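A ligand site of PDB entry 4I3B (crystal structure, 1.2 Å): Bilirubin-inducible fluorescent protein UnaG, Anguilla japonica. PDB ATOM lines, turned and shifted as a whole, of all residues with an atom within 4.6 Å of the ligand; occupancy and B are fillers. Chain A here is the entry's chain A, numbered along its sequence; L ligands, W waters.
An oxygen (O4) of the ligand sits at hydrogen-bond distance from the side-chain hydroxyl of Thr 61. The backbone NH of Ser 80 lies within hydrogen-bond range of an oxygen (O2) of the ligand (2.8 Å). The side-chain hydroxyl of Ser 80 sits at hydrogen-bond distance from an oxygen (O1) of the ligand. OH of Tyr 134 lies within hydrogen-bond range of O5 of the ligand (2.7 Å). The guanidinium group (NH1) of Arg 132 lies within salt-bridge range of an oxygen (O5) of the ligand (2.9 Å). The guanidinium group of Arg 112 lies within salt-bridge range of an oxygen (O6) of the ligand. A nitrogen (N3) of the ligand sits at hydrogen-bond distance from the side-chain amide oxygen (OD1) of Asn 57 (3.0 Å).
The backbone NH of Tyr 134 is in hydrogen-bond range of the backbone carbonyl oxygen of Leu 119, 2.8 Å away. The guanidinium group (NH2) of Arg 132 sits at hydrogen-bond distance from the side-chain hydroxyl (OG1) of Thr 37. O of Arg 132 lies within hydrogen-bond range of N of Val 121, 2.8 Å away. N of Val 53 sits at hydrogen-bond distance from O of Val 67 (2.8 Å). O of Tyr 99 sits at hydrogen-bond distance from N of Tyr 110, 2.8 Å away. The side-chain hydroxyl of Tyr 99 sits at hydrogen-bond distance from the side-chain carboxylate of Glu 77, at 2.7 Å. The backbone carbonyl oxygen (O) of Leu 21 is in hydrogen-bond range of the backbone NH (N) of Ala 26 (3.0 Å). OH of Tyr 110 lies within hydrogen-bond range of OH of Tyr 20.
Residues that only touch the ligand: Phe 5 (3.8 Å), Phe 17 (3.7 Å), Leu 21 (3.8 Å), Leu 30 (3.6 Å), Thr 37 (3.6 Å), Leu 41 (3.3 Å), Ile 43 (3.7 Å), Val 53 (3.7 Å), Ile 55 (3.4 Å), Leu 63 (3.98 Å), Thr 65 (3.8 Å), Val 67 (3.7 Å), Phe 69 (3.9 Å), Pro 79 (3.4 Å), Asp 81 (3.8 Å), Leu 97 (3.6 Å), Tyr 99 (3.7 Å), Tyr 110 (3.97 Å) and Leu 119 (3.4 Å). Hydrophobic or aromatic side chains that line the ligand: Phe 5, Phe 17, Leu 21, Leu 30, Leu 41, Ile 43, Val 53, Ile 55, Leu 63, Val 67, Phe 69, Pro 79, Leu 97, Tyr 99, Tyr 110, Leu 119 and Tyr 134. 25 residues have an atom within 4 Å of the ligand: Phe 5, Phe 17, Leu 21, Leu 30, Thr 37, Leu 41, Ile 43, Val 53, Ile 55, Asn 57, Thr 61, Leu 63, Thr 65, Val 67, Phe 69, Pro 79, Ser 80, Asp 81, Leu 97, Tyr 99, Tyr 110, Arg 112, Leu 119, Arg 132 and Tyr 134. The nearest printed residue that does not touch the ligand is Ala 26 (4.01 Å).
Water W4 bridges an oxygen (O6) of the ligand (2.8 Å) and the guanidinium group of Arg 112 (2.8 Å). Water W2 bridges the side-chain carboxylate of Asp 81 (2.8 Å) and an oxygen (O2) of the ligand (2.9 Å). Water W3 lies within hydrogen-bond range of OE2 of Glu 77 (2.7 Å) and O2 of the ligand (2.9 Å). Water W1 lies within hydrogen-bond range of the side-chain amide oxygen of Asn 57 (2.7 Å), the side-chain hydroxyl of Thr 37 (2.8 Å), the guanidinium group of Arg 132 (2.9 Å) and a nitrogen (N3) of the ligand (3.4 Å).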
ATOM      1  N   PHE A   5       8.229  23.655   0.213  1.00  0.00           N
ATOM      2  CA  PHE A   5       6.934  23.493   0.864  1.00  0.00           C
ATOM      3  C   PHE A   5       5.857  22.922  -0.070  1.00  0.00           C
ATOM      4  O   PHE A   5       4.795  22.501   0.409  1.00  0.00           O
ATOM      5  CB  PHE A   5       6.427  24.812   1.468  1.00  0.00           C
ATOM      6  CG  PHE A   5       7.273  25.332   2.595  1.00  0.00           C
ATOM      7  CD1 PHE A   5       7.169  24.816   3.885  1.00  0.00           C
ATOM      8  CD2 PHE A   5       8.182  26.338   2.358  1.00  0.00           C
ATOM      9  CE1 PHE A   5       7.961  25.306   4.925  1.00  0.00           C
ATOM     10  CE2 PHE A   5       8.989  26.850   3.378  1.00  0.00           C
ATOM     11  CZ  PHE A   5       8.884  26.328   4.676  1.00  0.00           C
ATOM     12  N   PHE A  17      -2.956  22.772  20.745  1.00  0.00           N
ATOM     13  CA  PHE A  17      -3.564  23.548  19.665  1.00  0.00           C
ATOM     14  C   PHE A  17      -4.898  24.187  20.105  1.00  0.00           C
ATOM     15  O   PHE A  17      -5.134  25.369  19.834  1.00  0.00           O
ATOM     16  CB  PHE A  17      -3.734  22.675  18.417  1.00  0.00           C
ATOM     17  CG  PHE A  17      -4.232  23.433  17.196  1.00  0.00           C
ATOM     18  CD1 PHE A  17      -3.682  24.649  16.812  1.00  0.00           C
ATOM     19  CD2 PHE A  17      -5.261  22.900  16.429  1.00  0.00           C
ATOM     20  CE1 PHE A  17      -4.157  25.298  15.686  1.00  0.00           C
ATOM     21  CE2 PHE A  17      -5.714  23.557  15.299  1.00  0.00           C
ATOM     22  CZ  PHE A  17      -5.172  24.766  14.946  1.00  0.00           C
ATOM     23  N   TYR A  20      -4.130  27.234  22.069  1.00  0.00           N
ATOM     24  CA  TYR A  20      -3.750  28.320  21.167  1.00  0.00           C
ATOM     25  C   TYR A  20      -5.004  28.940  20.544  1.00  0.00           C
ATOM     26  O   TYR A  20      -5.141  30.168  20.489  1.00  0.00           O
ATOM     27  CB  TYR A  20      -2.792  27.803  20.080  1.00  0.00           C
ATOM     28  CG  TYR A  20      -2.593  28.829  19.009  1.00  0.00           C
ATOM     29  CD1 TYR A  20      -1.681  29.858  19.173  1.00  0.00           C
ATOM     30  CD2 TYR A  20      -3.361  28.824  17.842  1.00  0.00           C
ATOM     31  CE1 TYR A  20      -1.529  30.823  18.191  1.00  0.00           C
ATOM     32  CE2 TYR A  20      -3.220  29.786  16.868  1.00  0.00           C
ATOM     33  CZ  TYR A  20      -2.318  30.775  17.040  1.00  0.00           C
ATOM     34  OH  TYR A  20      -2.202  31.734  16.050  1.00  0.00           O
ATOM     35  N   LEU A  21      -5.934  28.098  20.093  1.00  0.00           N
ATOM     36  CA  LEU A  21      -7.144  28.629  19.458  1.00  0.00           C
ATOM     37  C   LEU A  21      -7.977  29.459  20.449  1.00  0.00           C
ATOM     38  O   LEU A  21      -8.512  30.503  20.091  1.00  0.00           O
ATOM     39  CB  LEU A  21      -7.949  27.490  18.824  1.00  0.00           C
ATOM     40  CG  LEU A  21      -7.268  26.775  17.645  1.00  0.00           C
ATOM     41  CD1 LEU A  21      -8.161  25.639  17.193  1.00  0.00           C
ATOM     42  CD2 LEU A  21      -7.057  27.739  16.492  1.00  0.00           C
ATOM     43  N   ALA A  26     -11.007  32.091  19.634  1.00  0.00           N
ATOM     44  CA  ALA A  26     -11.987  31.182  19.056  1.00  0.00           C
ATOM     45  C   ALA A  26     -12.961  30.788  20.145  1.00  0.00           C
ATOM     46  O   ALA A  26     -12.556  30.581  21.304  1.00  0.00           O
ATOM     47  CB  ALA A  26     -11.290  29.938  18.509  1.00  0.00           C
ATOM     48  N   LEU A  30     -15.290  25.714  18.639  1.00  0.00           N
ATOM     49  CA  LEU A  30     -14.301  25.705  17.566  1.00  0.00           C
ATOM     50  C   LEU A  30     -12.884  25.433  18.059  1.00  0.00           C
ATOM     51  O   LEU A  30     -12.066  24.875  17.329  1.00  0.00           O
ATOM     52  CB  LEU A  30     -14.342  27.037  16.800  1.00  0.00           C
ATOM     53  CG  LEU A  30     -15.633  27.245  16.008  1.00  0.00           C
ATOM     54  CD1 LEU A  30     -15.527  28.537  15.249  1.00  0.00           C
ATOM     55  CD2 LEU A  30     -15.942  26.066  15.098  1.00  0.00           C
ATOM     56  N   GLY A  34     -11.302  22.354  16.610  1.00  0.00           N
ATOM     57  CA  GLY A  34     -10.026  22.532  15.932  1.00  0.00           C
ATOM     58  C   GLY A  34      -8.945  21.622  16.491  1.00  0.00           C
ATOM     59  O   GLY A  34      -8.136  21.036  15.751  1.00  0.00           O
ATOM     60  N   THR A  37      -9.051  18.229  14.857  1.00  0.00           N
ATOM     61  CA  THR A  37      -8.974  18.085  13.405  1.00  0.00           C
ATOM     62  C   THR A  37      -7.736  17.320  12.940  1.00  0.00           C
ATOM     63  O   THR A  37      -6.704  17.297  13.598  1.00  0.00           O
ATOM     64  CB  THR A  37      -9.000  19.449  12.675  1.00  0.00           C
ATOM     65  OG1 THR A  37      -7.954  20.309  13.161  1.00  0.00           O
ATOM     66  CG2 THR A  37     -10.352  20.117  12.862  1.00  0.00           C
ATOM     67  N   LEU A  41      -3.212  19.673   3.674  1.00  0.00           N
ATOM     68  CA  LEU A  41      -2.825  20.889   2.979  1.00  0.00           C
ATOM     69  C   LEU A  41      -2.395  20.563   1.570  1.00  0.00           C
ATOM     70  O   LEU A  41      -1.726  19.553   1.341  1.00  0.00           O
ATOM     71  CB  LEU A  41      -1.638  21.532   3.652  1.00  0.00           C
ATOM     72  CG  LEU A  41      -1.643  21.643   5.161  1.00  0.00           C
ATOM     73  CD1 LEU A  41      -0.322  22.184   5.669  1.00  0.00           C
ATOM     74  CD2 LEU A  41      -2.792  22.466   5.675  1.00  0.00           C
ATOM     75  N   ILE A  43      -0.301  22.696  -1.129  1.00  0.00           N
ATOM     76  CA  ILE A  43       0.473  23.909  -1.287  1.00  0.00           C
ATOM     77  C   ILE A  43       0.987  24.040  -2.716  1.00  0.00           C
ATOM     78  O   ILE A  43       1.548  23.104  -3.259  1.00  0.00           O
ATOM     79  CB  ILE A  43       1.638  23.889  -0.306  1.00  0.00           C
ATOM     80  CG1 ILE A  43       1.072  23.770   1.102  1.00  0.00           C
ATOM     81  CG2 ILE A  43       2.496  25.158  -0.443  1.00  0.00           C
ATOM     82  CD1 ILE A  43       2.106  23.908   2.226  1.00  0.00           C
ATOM     83  N   MET A  51       2.251  32.060  -3.245  1.00  0.00           N
ATOM     84  CA  MET A  51       1.778  30.758  -2.807  1.00  0.00           C
ATOM     85  C   MET A  51       0.276  30.708  -2.710  1.00  0.00           C
ATOM     86  O   MET A  51      -0.392  31.708  -2.451  1.00  0.00           O
ATOM     87  CB  MET A  51       2.369  30.395  -1.425  1.00  0.00           C
ATOM     88  CG  MET A  51       3.886  30.382  -1.430  1.00  0.00           C
ATOM     89  SD  MET A  51       4.630  29.968   0.161  1.00  0.00           S
ATOM     90  CE  MET A  51       4.093  28.278   0.410  1.00  0.00           C
ATOM     91  N   VAL A  53      -2.437  28.065  -0.617  1.00  0.00           N
ATOM     92  CA  VAL A  53      -2.584  26.918   0.270  1.00  0.00           C
ATOM     93  C   VAL A  53      -4.074  26.603   0.360  1.00  0.00           C
ATOM     94  O   VAL A  53      -4.877  27.478   0.753  1.00  0.00           O
ATOM     95  CB  VAL A  53      -1.993  27.163   1.674  1.00  0.00           C
ATOM     96  CG1 VAL A  53      -2.148  25.871   2.529  1.00  0.00           C
ATOM     97  CG2 VAL A  53      -0.526  27.512   1.570  1.00  0.00           C
ATOM     98  N   ILE A  55      -6.784  24.119   2.209  1.00  0.00           N
ATOM     99  CA  ILE A  55      -6.832  23.362   3.452  1.00  0.00           C
ATOM    100  C   ILE A  55      -8.171  22.661   3.581  1.00  0.00           C
ATOM    101  O   ILE A  55      -9.215  23.278   3.455  1.00  0.00           O
ATOM    102  CB  ILE A  55      -6.633  24.306   4.678  1.00  0.00           C
ATOM    103  CG1 ILE A  55      -5.325  25.113   4.549  1.00  0.00           C
ATOM    104  CG2 ILE A  55      -6.642  23.506   5.992  1.00  0.00           C
ATOM    105  CD1 ILE A  55      -5.475  26.485   3.965  1.00  0.00           C
ATOM    106  N   ASN A  57      -9.711  21.157   6.645  1.00  0.00           N
ATOM    107  CA  ASN A  57      -9.468  20.945   8.073  1.00  0.00           C
ATOM    108  C   ASN A  57      -9.977  19.589   8.532  1.00  0.00           C
ATOM    109  O   ASN A  57      -9.400  19.000   9.436  1.00  0.00           O
ATOM    110  CB  ASN A  57     -10.086  22.068   8.909  1.00  0.00           C
ATOM    111  CG  ASN A  57      -9.261  23.361   8.863  1.00  0.00           C
ATOM    112  OD1 ASN A  57      -8.151  23.408   9.404  1.00  0.00           O
ATOM    113  ND2 ASN A  57      -9.826  24.412   8.286  1.00  0.00           N
ATOM    114  N   THR A  61     -14.876  19.746  12.356  1.00  0.00           N
ATOM    115  CA  THR A  61     -15.319  21.090  11.989  1.00  0.00           C
ATOM    116  C   THR A  61     -15.786  21.136  10.535  1.00  0.00           C
ATOM    117  O   THR A  61     -16.654  21.918  10.184  1.00  0.00           O
ATOM    118  CB  THR A  61     -14.227  22.118  12.229  1.00  0.00           C
ATOM    119  OG1 THR A  61     -13.142  21.893  11.316  1.00  0.00           O
ATOM    120  CG2 THR A  61     -13.755  22.049  13.692  1.00  0.00           C
ATOM    121  N   LEU A  63     -14.407  22.338   7.870  1.00  0.00           N
ATOM    122  CA  LEU A  63     -14.167  23.588   7.177  1.00  0.00           C
ATOM    123  C   LEU A  63     -13.017  23.485   6.172  1.00  0.00           C
ATOM    124  O   LEU A  63     -11.900  23.158   6.539  1.00  0.00           O
ATOM    125  CB  LEU A  63     -13.836  24.677   8.210  1.00  0.00           C
ATOM    126  CG  LEU A  63     -14.982  24.987   9.168  1.00  0.00           C
ATOM    127  CD1 LEU A  63     -14.564  25.944  10.273  1.00  0.00           C
ATOM    128  CD2 LEU A  63     -16.203  25.502   8.421  1.00  0.00           C
ATOM    129  N   THR A  65     -10.836  25.791   3.407  1.00  0.00           N
ATOM    130  CA  THR A  65     -10.577  27.162   3.015  1.00  0.00           C
ATOM    131  C   THR A  65      -9.300  27.237   2.212  1.00  0.00           C
ATOM    132  O   THR A  65      -8.696  26.210   1.866  1.00  0.00           O
ATOM    133  CB  THR A  65     -10.528  28.091   4.257  1.00  0.00           C
ATOM    134  OG1 THR A  65     -10.575  29.452   3.822  1.00  0.00           O
ATOM    135  CG2 THR A  65      -9.278  27.872   5.086  1.00  0.00           C
ATOM    136  N   VAL A  67      -5.815  30.172   1.360  1.00  0.00           N
ATOM    137  CA  VAL A  67      -5.212  31.487   1.338  1.00  0.00           C
ATOM    138  C   VAL A  67      -4.307  31.587   0.115  1.00  0.00           C
ATOM    139  O   VAL A  67      -3.722  30.584  -0.338  1.00  0.00           O
ATOM    140  CB  VAL A  67      -4.391  31.786   2.613  1.00  0.00           C
ATOM    141  CG1 VAL A  67      -5.302  31.940   3.835  1.00  0.00           C
ATOM    142  CG2 VAL A  67      -3.321  30.750   2.855  1.00  0.00           C
ATOM    143  N   PHE A  69      -1.299  34.394  -1.400  1.00  0.00           N
ATOM    144  CA  PHE A  69      -0.523  35.569  -1.039  1.00  0.00           C
ATOM    145  C   PHE A  69       0.776  35.671  -1.821  1.00  0.00           C
ATOM    146  O   PHE A  69       1.278  34.689  -2.377  1.00  0.00           O
ATOM    147  CB  PHE A  69      -0.212  35.576   0.466  1.00  0.00           C
ATOM    148  CG  PHE A  69       0.473  34.310   0.946  1.00  0.00           C
ATOM    149  CD1 PHE A  69       1.860  34.186   0.862  1.00  0.00           C
ATOM    150  CD2 PHE A  69      -0.268  33.262   1.476  1.00  0.00           C
ATOM    151  CE1 PHE A  69       2.509  33.016   1.322  1.00  0.00           C
ATOM    152  CE2 PHE A  69       0.373  32.107   1.921  1.00  0.00           C
ATOM    153  CZ  PHE A  69       1.751  31.992   1.831  1.00  0.00           C
ATOM    154  N   GLU A  77      -7.535  38.269   5.613  1.00  0.00           N
ATOM    155  CA  GLU A  77      -7.864  36.878   5.861  1.00  0.00           C
ATOM    156  C   GLU A  77      -9.136  36.807   6.692  1.00  0.00           C
ATOM    157  O   GLU A  77      -9.412  37.668   7.524  1.00  0.00           O
ATOM    158  CB  GLU A  77      -6.700  36.183   6.596  1.00  0.00           C
ATOM    159  CG  GLU A  77      -6.824  34.646   6.678  1.00  0.00           C
ATOM    160  CD  GLU A  77      -5.617  33.986   7.344  1.00  0.00           C
ATOM    161  OE1 GLU A  77      -4.568  34.654   7.540  1.00  0.00           O
ATOM    162  OE2 GLU A  77      -5.725  32.787   7.687  1.00  0.00           O
ATOM    163  N   PRO A  79     -10.362  33.923   8.834  1.00  0.00           N
ATOM    164  CA  PRO A  79     -10.074  32.563   9.325  1.00  0.00           C
ATOM    165  C   PRO A  79     -11.270  31.892   9.997  1.00  0.00           C
ATOM    166  O   PRO A  79     -12.244  32.512  10.401  1.00  0.00           O
ATOM    167  CB  PRO A  79      -8.941  32.771  10.321  1.00  0.00           C
ATOM    168  CG  PRO A  79      -9.087  34.187  10.738  1.00  0.00           C
ATOM    169  CD  PRO A  79      -9.652  34.963   9.599  1.00  0.00           C
ATOM    170  N   SER A  80     -11.135  30.576  10.150  1.00  0.00           N
ATOM    171  CA  SER A  80     -12.183  29.717  10.707  1.00  0.00           C
ATOM    172  C   SER A  80     -12.515  30.041  12.135  1.00  0.00           C
ATOM    173  O   SER A  80     -13.587  29.654  12.626  1.00  0.00           O
ATOM    174  CB  SER A  80     -11.748  28.254  10.626  1.00  0.00           C
ATOM    175  OG  SER A  80     -11.668  27.830   9.279  1.00  0.00           O
ATOM    176  N   ASP A  81     -11.601  30.714  12.834  1.00  0.00           N
ATOM    177  CA  ASP A  81     -11.844  31.072  14.220  1.00  0.00           C
ATOM    178  C   ASP A  81     -12.748  32.290  14.359  1.00  0.00           C
ATOM    179  O   ASP A  81     -13.122  32.667  15.462  1.00  0.00           O
ATOM    180  CB  ASP A  81     -10.524  31.341  14.927  1.00  0.00           C
ATOM    181  CG  ASP A  81      -9.682  32.319  14.155  1.00  0.00           C
ATOM    182  OD1 ASP A  81     -10.114  33.476  14.112  1.00  0.00           O
ATOM    183  OD2 ASP A  81      -8.654  31.933  13.554  1.00  0.00           O
ATOM    184  N   LEU A  97       9.434  29.953   6.960  1.00  0.00           N
ATOM    185  CA  LEU A  97       8.357  30.787   6.445  1.00  0.00           C
ATOM    186  C   LEU A  97       7.602  31.283   7.656  1.00  0.00           C
ATOM    187  O   LEU A  97       7.113  30.473   8.466  1.00  0.00           O
ATOM    188  CB  LEU A  97       7.434  29.972   5.555  1.00  0.00           C
ATOM    189  CG  LEU A  97       6.435  30.757   4.749  1.00  0.00           C
ATOM    190  CD1 LEU A  97       7.153  31.538   3.625  1.00  0.00           C
ATOM    191  CD2 LEU A  97       5.398  29.771   4.234  1.00  0.00           C
ATOM    192  N   TYR A  99       4.582  33.677   9.251  1.00  0.00           N
ATOM    193  CA  TYR A  99       3.249  34.176   8.918  1.00  0.00           C
ATOM    194  C   TYR A  99       2.735  34.939  10.132  1.00  0.00           C
ATOM    195  O   TYR A  99       2.685  34.376  11.243  1.00  0.00           O
ATOM    196  CB  TYR A  99       2.392  32.945   8.622  1.00  0.00           C
ATOM    197  CG  TYR A  99       1.023  33.139   7.977  1.00  0.00           C
ATOM    198  CD1 TYR A  99       0.010  33.885   8.569  1.00  0.00           C
ATOM    199  CD2 TYR A  99       0.756  32.510   6.776  1.00  0.00           C
ATOM    200  CE1 TYR A  99      -1.291  33.976   7.953  1.00  0.00           C
ATOM    201  CE2 TYR A  99      -0.489  32.598   6.186  1.00  0.00           C
ATOM    202  CZ  TYR A  99      -1.503  33.318   6.760  1.00  0.00           C
ATOM    203  OH  TYR A  99      -2.725  33.362   6.127  1.00  0.00           O
ATOM    204  N   TYR A 110       2.995  32.330  13.159  1.00  0.00           N
ATOM    205  CA  TYR A 110       3.208  30.929  12.808  1.00  0.00           C
ATOM    206  C   TYR A 110       4.545  30.829  12.130  1.00  0.00           C
ATOM    207  O   TYR A 110       4.788  31.513  11.135  1.00  0.00           O
ATOM    208  CB  TYR A 110       2.140  30.439  11.834  1.00  0.00           C
ATOM    209  CG  TYR A 110       0.732  30.772  12.194  1.00  0.00           C
ATOM    210  CD1 TYR A 110       0.254  32.073  12.041  1.00  0.00           C
ATOM    211  CD2 TYR A 110      -0.131  29.796  12.680  1.00  0.00           C
ATOM    212  CE1 TYR A 110      -1.046  32.393  12.375  1.00  0.00           C
ATOM    213  CE2 TYR A 110      -1.434  30.109  13.008  1.00  0.00           C
ATOM    214  CZ  TYR A 110      -1.899  31.389  12.841  1.00  0.00           C
ATOM    215  OH  TYR A 110      -3.212  31.667  13.168  1.00  0.00           O
ATOM    216  N   ARG A 112       7.024  28.192  10.180  1.00  0.00           N
ATOM    217  CA  ARG A 112       6.972  26.930   9.463  1.00  0.00           C
ATOM    218  C   ARG A 112       8.342  26.578   8.889  1.00  0.00           C
ATOM    219  O   ARG A 112       9.021  27.397   8.274  1.00  0.00           O
ATOM    220  CB  ARG A 112       5.896  26.987   8.368  1.00  0.00           C
ATOM    221  CG  ARG A 112       4.496  27.018   8.979  1.00  0.00           C
ATOM    222  CD  ARG A 112       3.436  27.139   7.931  1.00  0.00           C
ATOM    223  NE  ARG A 112       2.100  27.056   8.500  1.00  0.00           N
ATOM    224  CZ  ARG A 112       1.255  28.064   8.689  1.00  0.00           C
ATOM    225  NH1 ARG A 112       1.571  29.327   8.408  1.00  0.00           N
ATOM    226  NH2 ARG A 112       0.065  27.801   9.188  1.00  0.00           N
ATOM    227  N   LEU A 119       6.715  18.922   7.856  1.00  0.00           N
ATOM    228  CA  LEU A 119       6.417  20.347   7.945  1.00  0.00           C
ATOM    229  C   LEU A 119       5.988  20.631   9.374  1.00  0.00           C
ATOM    230  O   LEU A 119       4.981  20.107   9.869  1.00  0.00           O
ATOM    231  CB  LEU A 119       5.317  20.725   6.946  1.00  0.00           C
ATOM    232  CG  LEU A 119       5.134  22.216   6.607  1.00  0.00           C
ATOM    233  CD1 LEU A 119       4.103  22.355   5.500  1.00  0.00           C
ATOM    234  CD2 LEU A 119       4.730  23.070   7.797  1.00  0.00           C
ATOM    235  N   VAL A 121       5.000  23.426  12.274  1.00  0.00           N
ATOM    236  CA  VAL A 121       4.507  24.787  12.537  1.00  0.00           C
ATOM    237  C   VAL A 121       4.514  25.037  14.048  1.00  0.00           C
ATOM    238  O   VAL A 121       3.941  24.255  14.798  1.00  0.00           O
ATOM    239  CB  VAL A 121       3.114  25.040  11.882  1.00  0.00           C
ATOM    240  CG1 VAL A 121       2.041  24.061  12.313  1.00  0.00           C
ATOM    241  CG2 VAL A 121       2.671  26.461  12.143  1.00  0.00           C
ATOM    242  N   LEU A 123       3.195  27.865  16.723  1.00  0.00           N
ATOM    243  CA  LEU A 123       2.182  28.889  16.811  1.00  0.00           C
ATOM    244  C   LEU A 123       2.314  29.606  18.128  1.00  0.00           C
ATOM    245  O   LEU A 123       2.330  28.972  19.192  1.00  0.00           O
ATOM    246  CB  LEU A 123       0.781  28.289  16.737  1.00  0.00           C
ATOM    247  CG  LEU A 123       0.447  27.363  15.563  1.00  0.00           C
ATOM    248  CD1 LEU A 123       0.966  25.893  15.706  1.00  0.00           C
ATOM    249  CD2 LEU A 123      -1.056  27.321  15.355  1.00  0.00           C
ATOM    250  N   ARG A 132       2.233  21.944  15.571  1.00  0.00           N
ATOM    251  CA  ARG A 132       1.686  20.872  14.757  1.00  0.00           C
ATOM    252  C   ARG A 132       2.747  20.439  13.764  1.00  0.00           C
ATOM    253  O   ARG A 132       3.601  21.234  13.381  1.00  0.00           O
ATOM    254  CB  ARG A 132       0.419  21.299  14.029  1.00  0.00           C
ATOM    255  CG  ARG A 132      -0.551  22.070  14.929  1.00  0.00           C
ATOM    256  CD  ARG A 132      -1.747  22.493  14.116  1.00  0.00           C
ATOM    257  NE  ARG A 132      -2.810  21.502  14.142  1.00  0.00           N
ATOM    258  CZ  ARG A 132      -3.922  21.553  13.386  1.00  0.00           C
ATOM    259  NH1 ARG A 132      -4.105  22.483  12.427  1.00  0.00           N
ATOM    260  NH2 ARG A 132      -4.865  20.667  13.573  1.00  0.00           N
ATOM    261  N   TYR A 134       3.234  17.972  10.085  1.00  0.00           N
ATOM    262  CA  TYR A 134       2.628  17.278   8.948  1.00  0.00           C
ATOM    263  C   TYR A 134       3.645  16.387   8.250  1.00  0.00           C
ATOM    264  O   TYR A 134       4.846  16.698   8.221  1.00  0.00           O
ATOM    265  CB  TYR A 134       2.108  18.278   7.927  1.00  0.00           C
ATOM    266  CG  TYR A 134       0.992  19.165   8.391  1.00  0.00           C
ATOM    267  CD1 TYR A 134       1.224  20.281   9.200  1.00  0.00           C
ATOM    268  CD2 TYR A 134      -0.286  18.954   7.915  1.00  0.00           C
ATOM    269  CE1 TYR A 134       0.162  21.113   9.566  1.00  0.00           C
ATOM    270  CE2 TYR A 134      -1.327  19.756   8.273  1.00  0.00           C
ATOM    271  CZ  TYR A 134      -1.101  20.857   9.071  1.00  0.00           C
ATOM    272  OH  TYR A 134      -2.168  21.651   9.421  1.00  0.00           O
HETATM  273  C1  LIG L   1      -4.577  24.892   9.100  1.00  0.00           C
HETATM  274  N1  LIG L   1      -2.971  26.182   7.634  1.00  0.00           N
HETATM  275  C2  LIG L   1      -4.234  25.978   8.096  1.00  0.00           C
HETATM  276  C3  LIG L   1      -5.061  26.967   7.589  1.00  0.00           C
HETATM  277  C4  LIG L   1      -4.253  27.804   6.811  1.00  0.00           C
HETATM  278  C5  LIG L   1      -2.967  27.291   6.857  1.00  0.00           C
HETATM  279  C6  LIG L   1      -4.692  29.011   6.047  1.00  0.00           C
HETATM  280  C7  LIG L   1      -6.535  27.081   7.820  1.00  0.00           C
HETATM  281  C8  LIG L   1      -6.878  28.123   8.818  1.00  0.00           C
HETATM  282  C9  LIG L   1      -8.343  28.276   9.028  1.00  0.00           C
HETATM  283  O1  LIG L   1      -9.137  27.316   8.812  1.00  0.00           O
HETATM  284  O2  LIG L   1      -8.744  29.436   9.399  1.00  0.00           O
HETATM  285  C10 LIG L   1      -1.813  27.884   6.138  1.00  0.00           C
HETATM  286  N2  LIG L   1      -0.223  26.011   6.217  1.00  0.00           N
HETATM  287  C11 LIG L   1      -0.604  27.320   5.843  1.00  0.00           C
HETATM  288  C12 LIG L   1       0.482  27.916   5.158  1.00  0.00           C
HETATM  289  C13 LIG L   1       1.463  27.106   5.050  1.00  0.00           C
HETATM  290  C14 LIG L   1       1.195  25.772   5.729  1.00  0.00           C
HETATM  291  C15 LIG L   1       0.414  29.325   4.619  1.00  0.00           C
HETATM  292  O3  LIG L   1       1.795  24.764   5.882  1.00  0.00           O
HETATM  293  C16 LIG L   1       2.769  27.339   4.389  1.00  0.00           C
HETATM  294  C17 LIG L   1       3.788  26.428   4.322  1.00  0.00           C
HETATM  295  N3  LIG L   1      -9.022  24.768  11.946  1.00  0.00           N
HETATM  296  C18 LIG L   1     -10.493  24.381  12.171  1.00  0.00           C
HETATM  297  C19 LIG L   1     -10.929  25.472  13.086  1.00  0.00           C
HETATM  298  C20 LIG L   1      -9.981  26.298  13.340  1.00  0.00           C
HETATM  299  C21 LIG L   1      -8.793  25.971  12.695  1.00  0.00           C
HETATM  300  C22 LIG L   1     -12.347  25.515  13.554  1.00  0.00           C
HETATM  301  O4  LIG L   1     -11.047  23.418  11.723  1.00  0.00           O
HETATM  302  C23 LIG L   1     -10.074  27.515  14.161  1.00  0.00           C
HETATM  303  C24 LIG L   1     -10.814  27.584  15.297  1.00  0.00           C
HETATM  304  C25 LIG L   1      -7.606  26.621  12.716  1.00  0.00           C
HETATM  305  N4  LIG L   1      -6.275  25.505  10.834  1.00  0.00           N
HETATM  306  C26 LIG L   1      -6.432  26.346  11.871  1.00  0.00           C
HETATM  307  C27 LIG L   1      -5.135  27.032  12.063  1.00  0.00           C
HETATM  308  C28 LIG L   1      -4.258  26.562  11.116  1.00  0.00           C
HETATM  309  C29 LIG L   1      -4.963  25.575  10.278  1.00  0.00           C
HETATM  310  C30 LIG L   1      -4.907  28.044  13.131  1.00  0.00           C
HETATM  311  C31 LIG L   1      -2.841  27.025  10.942  1.00  0.00           C
HETATM  312  C32 LIG L   1      -1.878  26.036  11.583  1.00  0.00           C
HETATM  313  C33 LIG L   1      -1.582  24.907  10.656  1.00  0.00           C
HETATM  314  O5  LIG L   1      -1.841  23.748  11.030  1.00  0.00           O
HETATM  315  O6  LIG L   1      -1.055  25.096   9.544  1.00  0.00           O
HETATM  316  O   HOH W   1      -6.847  22.201  11.427  1.00  0.00           O
HETATM  317  O   HOH W   2      -7.588  29.874  11.993  1.00  0.00           O
HETATM  318  O   HOH W   3      -7.805  31.121   7.178  1.00  0.00           O
HETATM  319  O   HOH W   4       1.514  24.301   8.712  1.00  0.00           O
HETATM  320  O   HOH W   5      -3.856  30.968   8.809  1.00  0.00           O
